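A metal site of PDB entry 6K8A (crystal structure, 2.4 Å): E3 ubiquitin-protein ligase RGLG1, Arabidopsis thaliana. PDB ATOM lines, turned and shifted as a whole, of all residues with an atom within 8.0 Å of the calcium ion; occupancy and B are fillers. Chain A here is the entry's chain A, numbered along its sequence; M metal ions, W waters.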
ATOM      1  N   SER A  37      -7.522   1.915 -17.425  1.00  0.00           N
ATOM      2  CA  SER A  37      -8.838   2.260 -16.949  1.00  0.00           C
ATOM      3  C   SER A  37      -9.827   1.318 -17.605  1.00  0.00           C
ATOM      4  O   SER A  37      -9.523   0.715 -18.638  1.00  0.00           O
ATOM      5  CB  SER A  37      -9.178   3.732 -17.231  1.00  0.00           C
ATOM      6  OG  SER A  37      -9.121   4.034 -18.613  1.00  0.00           O
ATOM      7  N   ASN A  38     -10.985   1.187 -16.965  1.00  0.00           N
ATOM      8  CA  ASN A  38     -12.063   0.341 -17.456  1.00  0.00           C
ATOM      9  C   ASN A  38     -13.390   1.059 -17.260  1.00  0.00           C
ATOM     10  O   ASN A  38     -13.518   1.900 -16.366  1.00  0.00           O
ATOM     11  CB  ASN A  38     -12.061  -1.020 -16.761  1.00  0.00           C
ATOM     12  CG  ASN A  38     -11.025  -1.969 -17.338  1.00  0.00           C
ATOM     13  OD1 ASN A  38     -11.284  -2.686 -18.304  1.00  0.00           O
ATOM     14  ND2 ASN A  38      -9.826  -1.975 -16.739  1.00  0.00           N
ATOM     15  N   LEU A  39     -14.374   0.741 -18.098  1.00  0.00           N
ATOM     16  CA  LEU A  39     -15.681   1.393 -18.031  1.00  0.00           C
ATOM     17  C   LEU A  39     -16.749   0.498 -17.403  1.00  0.00           C
ATOM     18  O   LEU A  39     -16.690  -0.737 -17.477  1.00  0.00           O
ATOM     19  CB  LEU A  39     -16.140   1.834 -19.408  1.00  0.00           C
ATOM     20  CG  LEU A  39     -15.291   2.896 -20.112  1.00  0.00           C
ATOM     21  CD1 LEU A  39     -15.835   3.113 -21.521  1.00  0.00           C
ATOM     22  CD2 LEU A  39     -15.249   4.186 -19.306  1.00  0.00           C
ATOM     23  N   ILE A  40     -17.715   1.133 -16.771  1.00  0.00           N
ATOM     24  CA  ILE A  40     -18.906   0.453 -16.299  1.00  0.00           C
ATOM     25  C   ILE A  40     -20.085   1.261 -16.783  1.00  0.00           C
ATOM     26  O   ILE A  40     -20.080   2.489 -16.673  1.00  0.00           O
ATOM     27  CB  ILE A  40     -18.944   0.328 -14.766  1.00  0.00           C
ATOM     28  CG1 ILE A  40     -17.637  -0.264 -14.230  1.00  0.00           C
ATOM     29  CG2 ILE A  40     -20.147  -0.500 -14.338  1.00  0.00           C
ATOM     30  CD1 ILE A  40     -17.552  -0.242 -12.730  1.00  0.00           C
ATOM     31  N   PHE A  86     -11.058   4.281 -23.346  1.00  0.00           N
ATOM     32  CA  PHE A  86     -10.901   4.302 -21.896  1.00  0.00           C
ATOM     33  C   PHE A  86     -11.328   3.001 -21.244  1.00  0.00           C
ATOM     34  O   PHE A  86     -11.374   2.912 -20.026  1.00  0.00           O
ATOM     35  CB  PHE A  86     -11.657   5.488 -21.307  1.00  0.00           C
ATOM     36  CG  PHE A  86     -11.032   6.802 -21.641  1.00  0.00           C
ATOM     37  CD1 PHE A  86     -11.298   7.423 -22.864  1.00  0.00           C
ATOM     38  CD2 PHE A  86     -10.124   7.403 -20.763  1.00  0.00           C
ATOM     39  CE1 PHE A  86     -10.691   8.646 -23.198  1.00  0.00           C
ATOM     40  CE2 PHE A  86      -9.512   8.610 -21.096  1.00  0.00           C
ATOM     41  CZ  PHE A  86      -9.800   9.237 -22.311  1.00  0.00           C
ATOM     42  N   ASP A  87     -11.634   1.985 -22.051  1.00  0.00           N
ATOM     43  CA  ASP A  87     -11.790   0.633 -21.505  1.00  0.00           C
ATOM     44  C   ASP A  87     -10.725  -0.278 -22.101  1.00  0.00           C
ATOM     45  O   ASP A  87     -10.822  -0.657 -23.269  1.00  0.00           O
ATOM     46  CB  ASP A  87     -13.176   0.082 -21.801  1.00  0.00           C
ATOM     47  CG  ASP A  87     -13.432  -1.201 -21.079  1.00  0.00           C
ATOM     48  OD1 ASP A  87     -13.799  -1.144 -19.881  1.00  0.00           O
ATOM     49  OD2 ASP A  87     -13.269  -2.275 -21.696  1.00  0.00           O
ATOM     50  N   GLU A  88      -9.726  -0.654 -21.313  1.00  0.00           N
ATOM     51  CA  GLU A  88      -8.486  -1.189 -21.877  1.00  0.00           C
ATOM     52  C   GLU A  88      -8.661  -2.509 -22.608  1.00  0.00           C
ATOM     53  O   GLU A  88      -7.892  -2.807 -23.522  1.00  0.00           O
ATOM     54  CB  GLU A  88      -7.437  -1.346 -20.786  1.00  0.00           C
ATOM     55  CG  GLU A  88      -7.914  -2.189 -19.660  1.00  0.00           C
ATOM     56  CD  GLU A  88      -6.878  -2.450 -18.598  1.00  0.00           C
ATOM     57  OE1 GLU A  88      -5.784  -1.820 -18.611  1.00  0.00           O
ATOM     58  OE2 GLU A  88      -7.185  -3.311 -17.744  1.00  0.00           O
ATOM     59  N   ASP A  89      -9.664  -3.308 -22.225  1.00  0.00           N
ATOM     60  CA  ASP A  89      -9.882  -4.630 -22.822  1.00  0.00           C
ATOM     61  C   ASP A  89     -11.175  -4.772 -23.655  1.00  0.00           C
ATOM     62  O   ASP A  89     -11.532  -5.884 -24.056  1.00  0.00           O
ATOM     63  CB  ASP A  89      -9.873  -5.717 -21.742  1.00  0.00           C
ATOM     64  CG  ASP A  89     -11.062  -5.623 -20.782  1.00  0.00           C
ATOM     65  OD1 ASP A  89     -11.885  -4.705 -20.895  1.00  0.00           O
ATOM     66  OD2 ASP A  89     -11.154  -6.478 -19.873  1.00  0.00           O
ATOM     67  N   ASN A  90     -11.874  -3.654 -23.888  1.00  0.00           N
ATOM     68  CA  ASN A  90     -13.077  -3.622 -24.725  1.00  0.00           C
ATOM     69  C   ASN A  90     -14.259  -4.475 -24.179  1.00  0.00           C
ATOM     70  O   ASN A  90     -15.247  -4.703 -24.884  1.00  0.00           O
ATOM     71  CB  ASN A  90     -12.712  -4.045 -26.145  1.00  0.00           C
ATOM     72  CG  ASN A  90     -13.692  -3.535 -27.201  1.00  0.00           C
ATOM     73  OD1 ASN A  90     -14.215  -2.412 -27.124  1.00  0.00           O
ATOM     74  ND2 ASN A  90     -13.945  -4.375 -28.203  1.00  0.00           N
ATOM     75  N   LEU A  91     -14.148  -4.943 -22.938  1.00  0.00           N
ATOM     76  CA  LEU A  91     -15.214  -5.708 -22.292  1.00  0.00           C
ATOM     77  C   LEU A  91     -15.914  -4.860 -21.251  1.00  0.00           C
ATOM     78  O   LEU A  91     -15.293  -4.423 -20.291  1.00  0.00           O
ATOM     79  CB  LEU A  91     -14.665  -6.976 -21.634  1.00  0.00           C
ATOM     80  CG  LEU A  91     -14.082  -8.073 -22.524  1.00  0.00           C
ATOM     81  CD1 LEU A  91     -13.975  -9.370 -21.750  1.00  0.00           C
ATOM     82  CD2 LEU A  91     -14.936  -8.265 -23.780  1.00  0.00           C
ATOM     83  N   ILE A  92     -17.204  -4.608 -21.429  1.00  0.00           N
ATOM     84  CA  ILE A  92     -17.872  -3.628 -20.598  1.00  0.00           C
ATOM     85  C   ILE A  92     -18.996  -4.252 -19.799  1.00  0.00           C
ATOM     86  O   ILE A  92     -19.942  -4.788 -20.360  1.00  0.00           O
ATOM     87  CB  ILE A  92     -18.429  -2.467 -21.469  1.00  0.00           C
ATOM     88  CG1 ILE A  92     -17.315  -1.817 -22.278  1.00  0.00           C
ATOM     89  CG2 ILE A  92     -19.122  -1.432 -20.608  1.00  0.00           C
ATOM     90  CD1 ILE A  92     -17.229  -2.317 -23.693  1.00  0.00           C
ATOM     91  N   PRO A  93     -18.886  -4.213 -18.461  1.00  0.00           N
ATOM     92  CA  PRO A  93     -20.028  -4.677 -17.657  1.00  0.00           C
ATOM     93  C   PRO A  93     -21.156  -3.656 -17.711  1.00  0.00           C
ATOM     94  O   PRO A  93     -20.915  -2.463 -17.481  1.00  0.00           O
ATOM     95  CB  PRO A  93     -19.456  -4.829 -16.238  1.00  0.00           C
ATOM     96  CG  PRO A  93     -18.229  -3.984 -16.213  1.00  0.00           C
ATOM     97  CD  PRO A  93     -17.709  -3.919 -17.634  1.00  0.00           C
ATOM     98  N   PHE A 116     -19.766 -10.198 -19.849  1.00  0.00           N
ATOM     99  CA  PHE A 116     -19.674  -8.799 -20.252  1.00  0.00           C
ATOM    100  C   PHE A 116     -19.954  -8.566 -21.745  1.00  0.00           C
ATOM    101  O   PHE A 116     -19.686  -9.432 -22.586  1.00  0.00           O
ATOM    102  CB  PHE A 116     -18.293  -8.236 -19.927  1.00  0.00           C
ATOM    103  CG  PHE A 116     -17.953  -8.209 -18.462  1.00  0.00           C
ATOM    104  CD1 PHE A 116     -18.940  -8.403 -17.493  1.00  0.00           C
ATOM    105  CD2 PHE A 116     -16.640  -7.983 -18.054  1.00  0.00           C
ATOM    106  CE1 PHE A 116     -18.623  -8.387 -16.140  1.00  0.00           C
ATOM    107  CE2 PHE A 116     -16.301  -7.967 -16.701  1.00  0.00           C
ATOM    108  CZ  PHE A 116     -17.297  -8.164 -15.742  1.00  0.00           C
ATOM    109  N   CYS A 117     -20.460  -7.383 -22.071  1.00  0.00           N
ATOM    110  CA  CYS A 117     -20.526  -6.942 -23.447  1.00  0.00           C
ATOM    111  C   CYS A 117     -19.147  -6.750 -24.065  1.00  0.00           C
ATOM    112  O   CYS A 117     -18.304  -6.036 -23.520  1.00  0.00           O
ATOM    113  CB  CYS A 117     -21.301  -5.638 -23.568  1.00  0.00           C
ATOM    114  SG  CYS A 117     -23.059  -5.835 -23.347  1.00  0.00           S
ATOM    115  N   HIS A 161     -11.777   2.836 -12.349  1.00  0.00           N
ATOM    116  CA  HIS A 161     -12.979   2.585 -13.161  1.00  0.00           C
ATOM    117  C   HIS A 161     -13.763   3.879 -13.367  1.00  0.00           C
ATOM    118  O   HIS A 161     -13.859   4.702 -12.456  1.00  0.00           O
ATOM    119  CB  HIS A 161     -13.901   1.533 -12.495  1.00  0.00           C
ATOM    120  CG  HIS A 161     -13.517   0.107 -12.749  1.00  0.00           C
ATOM    121  ND1 HIS A 161     -12.562  -0.562 -12.009  1.00  0.00           N
ATOM    122  CD2 HIS A 161     -13.985  -0.794 -13.651  1.00  0.00           C
ATOM    123  CE1 HIS A 161     -12.452  -1.801 -12.453  1.00  0.00           C
ATOM    124  NE2 HIS A 161     -13.306  -1.969 -13.448  1.00  0.00           N
HETATM  125 CA    CA M   1     -13.423  -3.419 -19.376  1.00  0.00          CA
HETATM  126  O   HOH W   1     -12.965  -5.295 -17.775  1.00  0.00           O
HETATM  127  O   HOH W   2     -14.635  -2.712 -17.462  1.00  0.00           O
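The side-chain carboxylate (OD1) of Asp 87 sits close to the backbone NH (N) of Leu 39, at 2.7 Å. The backbone NH (N) of Asn 90 sits close to the side-chain carboxylate (OD2) of Asp 87, at 2.9 Å. ND2 of Asn 38 is in hydrogen-bond range of OE2 of Glu 88 (3.1 Å).
The nearest printed residue that does not touch the calcium ion is Leu 39 (4.5 Å).
The calcium ion is bound by the backbone carbonyl oxygen (O) of Leu 91 (2.3 Å), the side-chain carboxylate (OD1) of Asp 87 (2.4 Å), water W2 (2.4 Å), the side-chain amide oxygen (OD1) of Asn 38 (2.5 Å), water W1 (2.5 Å), the side-chain carboxylate (OD1) of Asp 89 (2.5 Å) and the side-chain carboxylate (OD2) of Asp 87 (2.6 Å). The calcium ion has seven donor atoms within binding distance.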
